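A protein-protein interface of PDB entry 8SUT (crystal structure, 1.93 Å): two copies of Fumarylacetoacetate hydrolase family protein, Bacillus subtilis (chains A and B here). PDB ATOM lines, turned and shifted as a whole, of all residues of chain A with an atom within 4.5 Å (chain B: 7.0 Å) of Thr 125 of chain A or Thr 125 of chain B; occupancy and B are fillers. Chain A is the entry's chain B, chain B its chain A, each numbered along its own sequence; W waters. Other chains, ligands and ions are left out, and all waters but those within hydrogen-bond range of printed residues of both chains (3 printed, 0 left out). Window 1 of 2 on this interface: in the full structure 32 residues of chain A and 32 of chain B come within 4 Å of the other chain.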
ATOM      1  N   ASN A  96      23.487 -18.628 -30.929  1.00  0.00           N
ATOM      2  CA  ASN A  96      22.549 -17.729 -30.294  1.00  0.00           C
ATOM      3  C   ASN A  96      23.283 -16.744 -29.378  1.00  0.00           C
ATOM      4  O   ASN A  96      24.294 -17.065 -28.774  1.00  0.00           O
ATOM      5  CB  ASN A  96      21.505 -18.484 -29.512  1.00  0.00           C
ATOM      6  CG  ASN A  96      20.604 -19.390 -30.329  1.00  0.00           C
ATOM      7  OD1 ASN A  96      20.916 -19.791 -31.436  1.00  0.00           O
ATOM      8  ND2 ASN A  96      19.495 -19.769 -29.745  1.00  0.00           N
ATOM      9  N   ILE A  97      22.759 -15.519 -29.318  1.00  0.00           N
ATOM     10  CA  ILE A  97      23.205 -14.537 -28.345  1.00  0.00           C
ATOM     11  C   ILE A  97      22.905 -15.046 -26.937  1.00  0.00           C
ATOM     12  O   ILE A  97      21.796 -15.496 -26.640  1.00  0.00           O
ATOM     13  CB  ILE A  97      22.527 -13.187 -28.679  1.00  0.00           C
ATOM     14  CG1 ILE A  97      22.999 -12.717 -30.084  1.00  0.00           C
ATOM     15  CG2 ILE A  97      22.776 -12.130 -27.608  1.00  0.00           C
ATOM     16  CD1 ILE A  97      22.223 -11.878 -30.655  1.00  0.00           C
ATOM     17  N   PHE A 124      19.827 -17.384 -20.724  1.00  0.00           N
ATOM     18  CA  PHE A 124      19.051 -17.904 -21.835  1.00  0.00           C
ATOM     19  C   PHE A 124      19.640 -17.337 -23.128  1.00  0.00           C
ATOM     20  O   PHE A 124      20.670 -16.665 -23.103  1.00  0.00           O
ATOM     21  CB  PHE A 124      17.568 -17.547 -21.643  1.00  0.00           C
ATOM     22  CG  PHE A 124      17.377 -16.055 -21.577  1.00  0.00           C
ATOM     23  CD1 PHE A 124      17.533 -15.374 -20.379  1.00  0.00           C
ATOM     24  CD2 PHE A 124      17.120 -15.323 -22.727  1.00  0.00           C
ATOM     25  CE1 PHE A 124      17.396 -13.998 -20.327  1.00  0.00           C
ATOM     26  CE2 PHE A 124      16.980 -13.950 -22.674  1.00  0.00           C
ATOM     27  CZ  PHE A 124      17.120 -13.297 -21.472  1.00  0.00           C
ATOM     28  N   THR A 125      18.981 -17.613 -24.262  1.00  0.00           N
ATOM     29  CA  THR A 125      19.471 -17.189 -25.561  1.00  0.00           C
ATOM     30  C   THR A 125      18.434 -16.564 -26.494  1.00  0.00           C
ATOM     31  O   THR A 125      17.233 -16.780 -26.356  1.00  0.00           O
ATOM     32  CB  THR A 125      20.132 -18.369 -26.302  1.00  0.00           C
ATOM     33  OG1 THR A 125      19.121 -19.261 -26.785  1.00  0.00           O
ATOM     34  CG2 THR A 125      21.127 -19.117 -25.442  1.00  0.00           C
ATOM     35  N   LYS A 126      18.955 -15.781 -27.446  1.00  0.00           N
ATOM     36  CA  LYS A 126      18.215 -15.274 -28.590  1.00  0.00           C
ATOM     37  C   LYS A 126      18.809 -15.871 -29.860  1.00  0.00           C
ATOM     38  O   LYS A 126      20.011 -15.753 -30.091  1.00  0.00           O
ATOM     39  CB  LYS A 126      18.320 -13.748 -28.724  1.00  0.00           C
ATOM     40  CG  LYS A 126      17.814 -12.991 -27.550  1.00  0.00           C
ATOM     41  CD  LYS A 126      17.988 -11.493 -27.686  1.00  0.00           C
ATOM     42  CE  LYS A 126      16.942 -10.794 -28.563  1.00  0.00           C
ATOM     43  NZ  LYS A 126      15.580 -10.692 -27.954  1.00  0.00           N
ATOM     44  N   SER A 127      17.937 -16.438 -30.700  1.00  0.00           N
ATOM     45  CA  SER A 127      18.306 -16.933 -32.005  1.00  0.00           C
ATOM     46  C   SER A 127      18.997 -15.861 -32.844  1.00  0.00           C
ATOM     47  O   SER A 127      18.664 -14.684 -32.734  1.00  0.00           O
ATOM     48  CB  SER A 127      17.085 -17.431 -32.761  1.00  0.00           C
ATOM     49  OG  SER A 127      17.454 -17.799 -34.077  1.00  0.00           O
ATOM     50  N   PHE A 196      13.201 -18.736 -24.547  1.00  0.00           N
ATOM     51  CA  PHE A 196      13.644 -18.785 -25.929  1.00  0.00           C
ATOM     52  C   PHE A 196      12.640 -18.237 -26.951  1.00  0.00           C
ATOM     53  O   PHE A 196      12.976 -17.353 -27.738  1.00  0.00           O
ATOM     54  CB  PHE A 196      14.052 -20.227 -26.296  1.00  0.00           C
ATOM     55  CG  PHE A 196      14.421 -20.343 -27.748  1.00  0.00           C
ATOM     56  CD1 PHE A 196      15.571 -19.737 -28.241  1.00  0.00           C
ATOM     57  CD2 PHE A 196      13.580 -20.984 -28.642  1.00  0.00           C
ATOM     58  CE1 PHE A 196      15.896 -19.835 -29.595  1.00  0.00           C
ATOM     59  CE2 PHE A 196      13.903 -21.069 -29.992  1.00  0.00           C
ATOM     60  CZ  PHE A 196      15.068 -20.515 -30.456  1.00  0.00           C
ATOM     61  N   LYS A 199      11.931 -14.505 -26.682  1.00  0.00           N
ATOM     62  CA  LYS A 199      13.154 -13.777 -26.948  1.00  0.00           C
ATOM     63  C   LYS A 199      13.648 -13.865 -28.389  1.00  0.00           C
ATOM     64  O   LYS A 199      14.524 -13.100 -28.774  1.00  0.00           O
ATOM     65  CB  LYS A 199      14.257 -14.305 -26.015  1.00  0.00           C
ATOM     66  CG  LYS A 199      14.034 -13.996 -24.549  1.00  0.00           C
ATOM     67  CD  LYS A 199      14.273 -12.559 -24.233  1.00  0.00           C
ATOM     68  CE  LYS A 199      14.083 -12.262 -22.764  1.00  0.00           C
ATOM     69  NZ  LYS A 199      14.492 -10.874 -22.425  1.00  0.00           N
ATOM     70  N   SER A 200      13.074 -14.770 -29.186  1.00  0.00           N
ATOM     71  CA  SER A 200      13.634 -15.076 -30.492  1.00  0.00           C
ATOM     72  C   SER A 200      12.743 -14.791 -31.694  1.00  0.00           C
ATOM     73  O   SER A 200      12.854 -15.449 -32.722  1.00  0.00           O
ATOM     74  CB  SER A 200      14.059 -16.532 -30.542  1.00  0.00           C
ATOM     75  OG  SER A 200      15.123 -16.707 -29.621  1.00  0.00           O
ATOM     76  N   LYS B  95      22.928 -22.432 -35.687  1.00  0.00           N
ATOM     77  CA  LYS B  95      22.339 -21.866 -34.495  1.00  0.00           C
ATOM     78  C   LYS B  95      22.194 -22.967 -33.460  1.00  0.00           C
ATOM     79  O   LYS B  95      22.543 -24.100 -33.728  1.00  0.00           O
ATOM     80  CB  LYS B  95      21.020 -21.169 -34.786  1.00  0.00           C
ATOM     81  CG  LYS B  95      19.983 -21.975 -35.484  1.00  0.00           C
ATOM     82  CD  LYS B  95      18.726 -21.118 -35.801  1.00  0.00           C
ATOM     83  CE  LYS B  95      18.917 -20.045 -36.872  1.00  0.00           C
ATOM     84  NZ  LYS B  95      19.258 -20.596 -38.234  1.00  0.00           N
ATOM     85  N   ASN B  96      21.793 -22.590 -32.250  1.00  0.00           N
ATOM     86  CA  ASN B  96      21.609 -23.568 -31.189  1.00  0.00           C
ATOM     87  C   ASN B  96      20.539 -24.579 -31.600  1.00  0.00           C
ATOM     88  O   ASN B  96      19.590 -24.237 -32.305  1.00  0.00           O
ATOM     89  CB  ASN B  96      21.241 -22.916 -29.902  1.00  0.00           C
ATOM     90  CG  ASN B  96      22.298 -21.993 -29.316  1.00  0.00           C
ATOM     91  OD1 ASN B  96      23.218 -21.522 -29.999  1.00  0.00           O
ATOM     92  ND2 ASN B  96      22.131 -21.692 -28.025  1.00  0.00           N
ATOM     93  N   ILE B  97      20.733 -25.826 -31.166  1.00  0.00           N
ATOM     94  CA  ILE B  97      19.719 -26.860 -31.260  1.00  0.00           C
ATOM     95  C   ILE B  97      18.477 -26.426 -30.493  1.00  0.00           C
ATOM     96  O   ILE B  97      18.575 -26.008 -29.337  1.00  0.00           O
ATOM     97  CB  ILE B  97      20.273 -28.191 -30.687  1.00  0.00           C
ATOM     98  CG1 ILE B  97      21.661 -28.558 -31.298  1.00  0.00           C
ATOM     99  CG2 ILE B  97      19.244 -29.300 -30.787  1.00  0.00           C
ATOM    100  CD1 ILE B  97      21.695 -28.659 -32.554  1.00  0.00           C
ATOM    101  N   ILE B  98      17.314 -26.515 -31.147  1.00  0.00           N
ATOM    102  CA  ILE B  98      16.054 -26.185 -30.504  1.00  0.00           C
ATOM    103  C   ILE B  98      15.491 -27.431 -29.833  1.00  0.00           C
ATOM    104  O   ILE B  98      15.260 -28.442 -30.513  1.00  0.00           O
ATOM    105  CB  ILE B  98      15.064 -25.598 -31.516  1.00  0.00           C
ATOM    106  CG1 ILE B  98      15.625 -24.318 -32.151  1.00  0.00           C
ATOM    107  CG2 ILE B  98      13.720 -25.363 -30.874  1.00  0.00           C
ATOM    108  CD1 ILE B  98      14.892 -23.949 -33.454  1.00  0.00           C
ATOM    109  N   CYS B  99      15.287 -27.342 -28.511  1.00  0.00           N
ATOM    110  CA  CYS B  99      14.884 -28.485 -27.699  1.00  0.00           C
ATOM    111  C   CYS B  99      13.510 -28.262 -27.083  1.00  0.00           C
ATOM    112  O   CYS B  99      13.211 -27.169 -26.588  1.00  0.00           O
ATOM    113  CB  CYS B  99      15.897 -28.762 -26.607  1.00  0.00           C
ATOM    114  SG  CYS B  99      17.547 -29.119 -27.204  1.00  0.00           S
ATOM    115  N   VAL B 123      10.236 -24.532 -24.755  1.00  0.00           N
ATOM    116  CA  VAL B 123      11.303 -24.548 -25.741  1.00  0.00           C
ATOM    117  C   VAL B 123      12.558 -23.864 -25.203  1.00  0.00           C
ATOM    118  O   VAL B 123      12.500 -22.743 -24.703  1.00  0.00           O
ATOM    119  CB  VAL B 123      10.816 -23.883 -27.025  1.00  0.00           C
ATOM    120  CG1 VAL B 123      11.846 -24.040 -28.133  1.00  0.00           C
ATOM    121  CG2 VAL B 123       9.447 -24.438 -27.440  1.00  0.00           C
ATOM    122  N   PHE B 124      13.685 -24.581 -25.273  1.00  0.00           N
ATOM    123  CA  PHE B 124      14.980 -24.040 -24.902  1.00  0.00           C
ATOM    124  C   PHE B 124      16.006 -24.492 -25.945  1.00  0.00           C
ATOM    125  O   PHE B 124      15.650 -25.131 -26.938  1.00  0.00           O
ATOM    126  CB  PHE B 124      15.326 -24.479 -23.468  1.00  0.00           C
ATOM    127  CG  PHE B 124      15.397 -25.971 -23.367  1.00  0.00           C
ATOM    128  CD1 PHE B 124      14.251 -26.721 -23.146  1.00  0.00           C
ATOM    129  CD2 PHE B 124      16.591 -26.634 -23.567  1.00  0.00           C
ATOM    130  CE1 PHE B 124      14.314 -28.100 -23.078  1.00  0.00           C
ATOM    131  CE2 PHE B 124      16.648 -28.015 -23.512  1.00  0.00           C
ATOM    132  CZ  PHE B 124      15.506 -28.740 -23.273  1.00  0.00           C
ATOM    133  N   THR B 125      17.285 -24.164 -25.725  1.00  0.00           N
ATOM    134  CA  THR B 125      18.336 -24.498 -26.672  1.00  0.00           C
ATOM    135  C   THR B 125      19.617 -25.107 -26.101  1.00  0.00           C
ATOM    136  O   THR B 125      19.905 -24.968 -24.915  1.00  0.00           O
ATOM    137  CB  THR B 125      18.729 -23.260 -27.500  1.00  0.00           C
ATOM    138  OG1 THR B 125      19.510 -22.370 -26.700  1.00  0.00           O
ATOM    139  CG2 THR B 125      17.512 -22.531 -28.072  1.00  0.00           C
ATOM    140  N   LYS B 126      20.345 -25.818 -26.979  1.00  0.00           N
ATOM    141  CA  LYS B 126      21.698 -26.293 -26.726  1.00  0.00           C
ATOM    142  C   LYS B 126      22.673 -25.598 -27.669  1.00  0.00           C
ATOM    143  O   LYS B 126      22.489 -25.648 -28.887  1.00  0.00           O
ATOM    144  CB  LYS B 126      21.849 -27.794 -26.967  1.00  0.00           C
ATOM    145  CG  LYS B 126      20.965 -28.647 -26.108  1.00  0.00           C
ATOM    146  CD  LYS B 126      21.088 -30.131 -26.439  1.00  0.00           C
ATOM    147  CE  LYS B 126      22.299 -30.828 -25.816  1.00  0.00           C
ATOM    148  NZ  LYS B 126      22.212 -31.029 -24.352  1.00  0.00           N
ATOM    149  N   SER B 127      23.737 -25.009 -27.097  1.00  0.00           N
ATOM    150  CA  SER B 127      24.803 -24.427 -27.896  1.00  0.00           C
ATOM    151  C   SER B 127      25.387 -25.423 -28.898  1.00  0.00           C
ATOM    152  O   SER B 127      25.461 -26.620 -28.615  1.00  0.00           O
ATOM    153  CB  SER B 127      25.911 -23.887 -27.002  1.00  0.00           C
ATOM    154  OG  SER B 127      27.013 -23.479 -27.804  1.00  0.00           O
ATOM    155  N   ASP B 182      20.217 -35.723 -25.609  1.00  0.00           N
ATOM    156  CA  ASP B 182      20.189 -34.412 -24.979  1.00  0.00           C
ATOM    157  C   ASP B 182      20.724 -34.508 -23.549  1.00  0.00           C
ATOM    158  O   ASP B 182      19.977 -34.415 -22.581  1.00  0.00           O
ATOM    159  CB  ASP B 182      18.756 -33.851 -25.017  1.00  0.00           C
ATOM    160  CG  ASP B 182      18.540 -32.508 -24.333  1.00  0.00           C
ATOM    161  OD1 ASP B 182      19.544 -31.806 -24.033  1.00  0.00           O
ATOM    162  OD2 ASP B 182      17.397 -32.166 -24.091  1.00  0.00           O
ATOM    163  N   GLN B 194      16.642 -21.040 -16.127  1.00  0.00           N
ATOM    164  CA  GLN B 194      16.607 -21.310 -17.552  1.00  0.00           C
ATOM    165  C   GLN B 194      17.598 -22.454 -17.781  1.00  0.00           C
ATOM    166  O   GLN B 194      18.614 -22.547 -17.103  1.00  0.00           O
ATOM    167  CB  GLN B 194      16.921 -20.027 -18.330  1.00  0.00           C
ATOM    168  CG  GLN B 194      15.892 -18.901 -18.113  1.00  0.00           C
ATOM    169  CD  GLN B 194      14.570 -19.172 -18.770  1.00  0.00           C
ATOM    170  OE1 GLN B 194      14.485 -19.469 -19.965  1.00  0.00           O
ATOM    171  NE2 GLN B 194      13.485 -19.079 -18.022  1.00  0.00           N
ATOM    172  N   PHE B 195      17.264 -23.335 -18.732  1.00  0.00           N
ATOM    173  CA  PHE B 195      17.966 -24.589 -18.947  1.00  0.00           C
ATOM    174  C   PHE B 195      19.268 -24.497 -19.734  1.00  0.00           C
ATOM    175  O   PHE B 195      20.042 -25.457 -19.759  1.00  0.00           O
ATOM    176  CB  PHE B 195      17.016 -25.553 -19.688  1.00  0.00           C
ATOM    177  CG  PHE B 195      15.844 -26.086 -18.901  1.00  0.00           C
ATOM    178  CD1 PHE B 195      15.722 -25.833 -17.533  1.00  0.00           C
ATOM    179  CD2 PHE B 195      14.866 -26.841 -19.518  1.00  0.00           C
ATOM    180  CE1 PHE B 195      14.642 -26.340 -16.807  1.00  0.00           C
ATOM    181  CE2 PHE B 195      13.783 -27.340 -18.791  1.00  0.00           C
ATOM    182  CZ  PHE B 195      13.680 -27.085 -17.443  1.00  0.00           C
ATOM    183  N   PHE B 196      19.508 -23.347 -20.380  1.00  0.00           N
ATOM    184  CA  PHE B 196      20.606 -23.211 -21.316  1.00  0.00           C
ATOM    185  C   PHE B 196      21.946 -23.713 -20.768  1.00  0.00           C
ATOM    186  O   PHE B 196      22.596 -24.529 -21.411  1.00  0.00           O
ATOM    187  CB  PHE B 196      20.691 -21.757 -21.791  1.00  0.00           C
ATOM    188  CG  PHE B 196      21.938 -21.480 -22.581  1.00  0.00           C
ATOM    189  CD1 PHE B 196      22.087 -21.980 -23.854  1.00  0.00           C
ATOM    190  CD2 PHE B 196      22.994 -20.774 -22.016  1.00  0.00           C
ATOM    191  CE1 PHE B 196      23.269 -21.759 -24.575  1.00  0.00           C
ATOM    192  CE2 PHE B 196      24.162 -20.552 -22.729  1.00  0.00           C
ATOM    193  CZ  PHE B 196      24.291 -21.045 -24.010  1.00  0.00           C
ATOM    194  N   ILE B 197      22.367 -23.253 -19.584  1.00  0.00           N
ATOM    195  CA  ILE B 197      23.675 -23.645 -19.083  1.00  0.00           C
ATOM    196  C   ILE B 197      23.805 -25.146 -18.800  1.00  0.00           C
ATOM    197  O   ILE B 197      24.812 -25.759 -19.146  1.00  0.00           O
ATOM    198  CB  ILE B 197      24.071 -22.784 -17.845  1.00  0.00           C
ATOM    199  CG1 ILE B 197      24.468 -21.384 -18.311  1.00  0.00           C
ATOM    200  CG2 ILE B 197      25.198 -23.429 -17.055  1.00  0.00           C
ATOM    201  CD1 ILE B 197      24.914 -20.499 -17.271  1.00  0.00           C
ATOM    202  N   LYS B 199      22.140 -27.482 -20.190  1.00  0.00           N
ATOM    203  CA  LYS B 199      22.000 -28.148 -21.472  1.00  0.00           C
ATOM    204  C   LYS B 199      23.173 -27.938 -22.432  1.00  0.00           C
ATOM    205  O   LYS B 199      23.260 -28.631 -23.447  1.00  0.00           O
ATOM    206  CB  LYS B 199      20.721 -27.632 -22.153  1.00  0.00           C
ATOM    207  CG  LYS B 199      19.438 -28.017 -21.443  1.00  0.00           C
ATOM    208  CD  LYS B 199      19.116 -29.460 -21.656  1.00  0.00           C
ATOM    209  CE  LYS B 199      17.837 -29.857 -20.974  1.00  0.00           C
ATOM    210  NZ  LYS B 199      17.451 -31.217 -21.354  1.00  0.00           N
ATOM    211  N   SER B 200      24.082 -27.006 -22.109  1.00  0.00           N
ATOM    212  CA  SER B 200      25.090 -26.585 -23.072  1.00  0.00           C
ATOM    213  C   SER B 200      26.543 -26.848 -22.697  1.00  0.00           C
ATOM    214  O   SER B 200      27.435 -26.152 -23.166  1.00  0.00           O
ATOM    215  CB  SER B 200      24.924 -25.114 -23.404  1.00  0.00           C
ATOM    216  OG  SER B 200      23.689 -24.939 -24.062  1.00  0.00           O
HETATM  217  O   HOH W   1      17.664 -20.898 -24.375  1.00  0.00           O
HETATM  218  O   HOH W   2      24.476 -19.748 -27.604  1.00  0.00           O
HETATM  219  O   HOH W   3      18.319 -21.719 -31.865  1.00  0.00           O
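The side-chain amide oxygen (OD1) of Asn 96 of chain A is in hydrogen-bond range of the backbone NH (N) of Asn 96 of chain B, at 3.0 Å. OG1 of Thr 125 of chain A is in hydrogen-bond range of OG1 of Thr 125 of chain B, at 3.1 Å.
Among the printed residues, pairs that only touch across the chains: Asn 96 of chain A with Lys 95 of chain B, Asn 96 of chain A with Thr 125 of chain B, Thr 125 of chain A with Asn 96 of chain B, Thr 125 of chain A with Phe 196 of chain B, Ser 127 of chain A with Lys 95 of chain B, Phe 196 of chain A with Val 123 of chain B and Phe 196 of chain A with Thr 125 of chain B.
Water W3 bridges O of Asn 96 of chain B and ND2 of Asn 96 of chain A. Water W2 bridges the backbone carbonyl oxygen of Asn 96 of chain A (2.9 Å) and the side-chain amide nitrogen of Asn 96 of chain B (3.1 Å). Water W1 bridges OG1 of Thr 125 of chain A (3.3 Å) and OG1 of Thr 125 of chain B (3.3 Å).
Asn 96 of chain A touches its own counterpart, Asn 96 of chain B. Asn 96 of chain A touches Thr 125 of chain B, and with the chains exchanged Thr 125 of chain A touches Asn 96 of chain B. Thr 125 of chain B touches its own counterpart, Thr 125 of chain A. Thr 125 of chain A touches Phe 196 of chain B, and with the chains exchanged Phe 196 of chain A touches Thr 125 of chain B. Of the 9 pairs that touch across the chains among the printed residues, 6 have their exchanged pair printed and touching as well.
OG1 of Thr 125 of chain B sits at hydrogen-bond distance from ND2 of Asn 96 of chain B, 3.0 Å away. O of Phe 196 of chain B sits at hydrogen-bond distance from OG of Ser 200 of chain B, at 2.9 Å. OG1 of Thr 125 of chain A is in hydrogen-bond range of ND2 of Asn 96 of chain A (3.0 Å). N of Ser 127 of chain A is in hydrogen-bond range of OG of Ser 200 of chain A (3.0 Å). The backbone carbonyl oxygen (O) of Phe 196 of chain A is in hydrogen-bond range of the side-chain hydroxyl (OG) of Ser 200 of chain A (2.9 Å).
Of chain B, only Asn 96, Thr 125 and Phe 196 come within 4 Å of Thr 125 of chain A. Thr 125 of chain B touches just these residues of chain A: Asn 96 (3.8 Å), Thr 125 (3.1 Å) and Phe 196 (3.4 Å). Of the printed residues of chain A, Asn 96 of chain B touches Asn 96 (3.0 Å) and Thr 125 (3.8 Å). Printed residues of chain B within 4 Å of Phe 196 of chain A: Val 123 and Thr 125. Of the printed residues of chain A, Lys 95 of chain B touches Asn 96 and Ser 127. The nearest residue of chain B that does not touch Thr 125 of chain A is Phe 124 of chain B (6.1 Å). The nearest printed residue of chain A that does not touch Val 123 of chain B is Thr 125 of chain A (7.8 Å).
Of the 17 printed residues of chain B, 5 touch a printed residue of chain A. Among the printed residues, no Asp or Glu carboxylate lies within 4 Å of a Lys or Arg side-chain nitrogen of the other chain.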
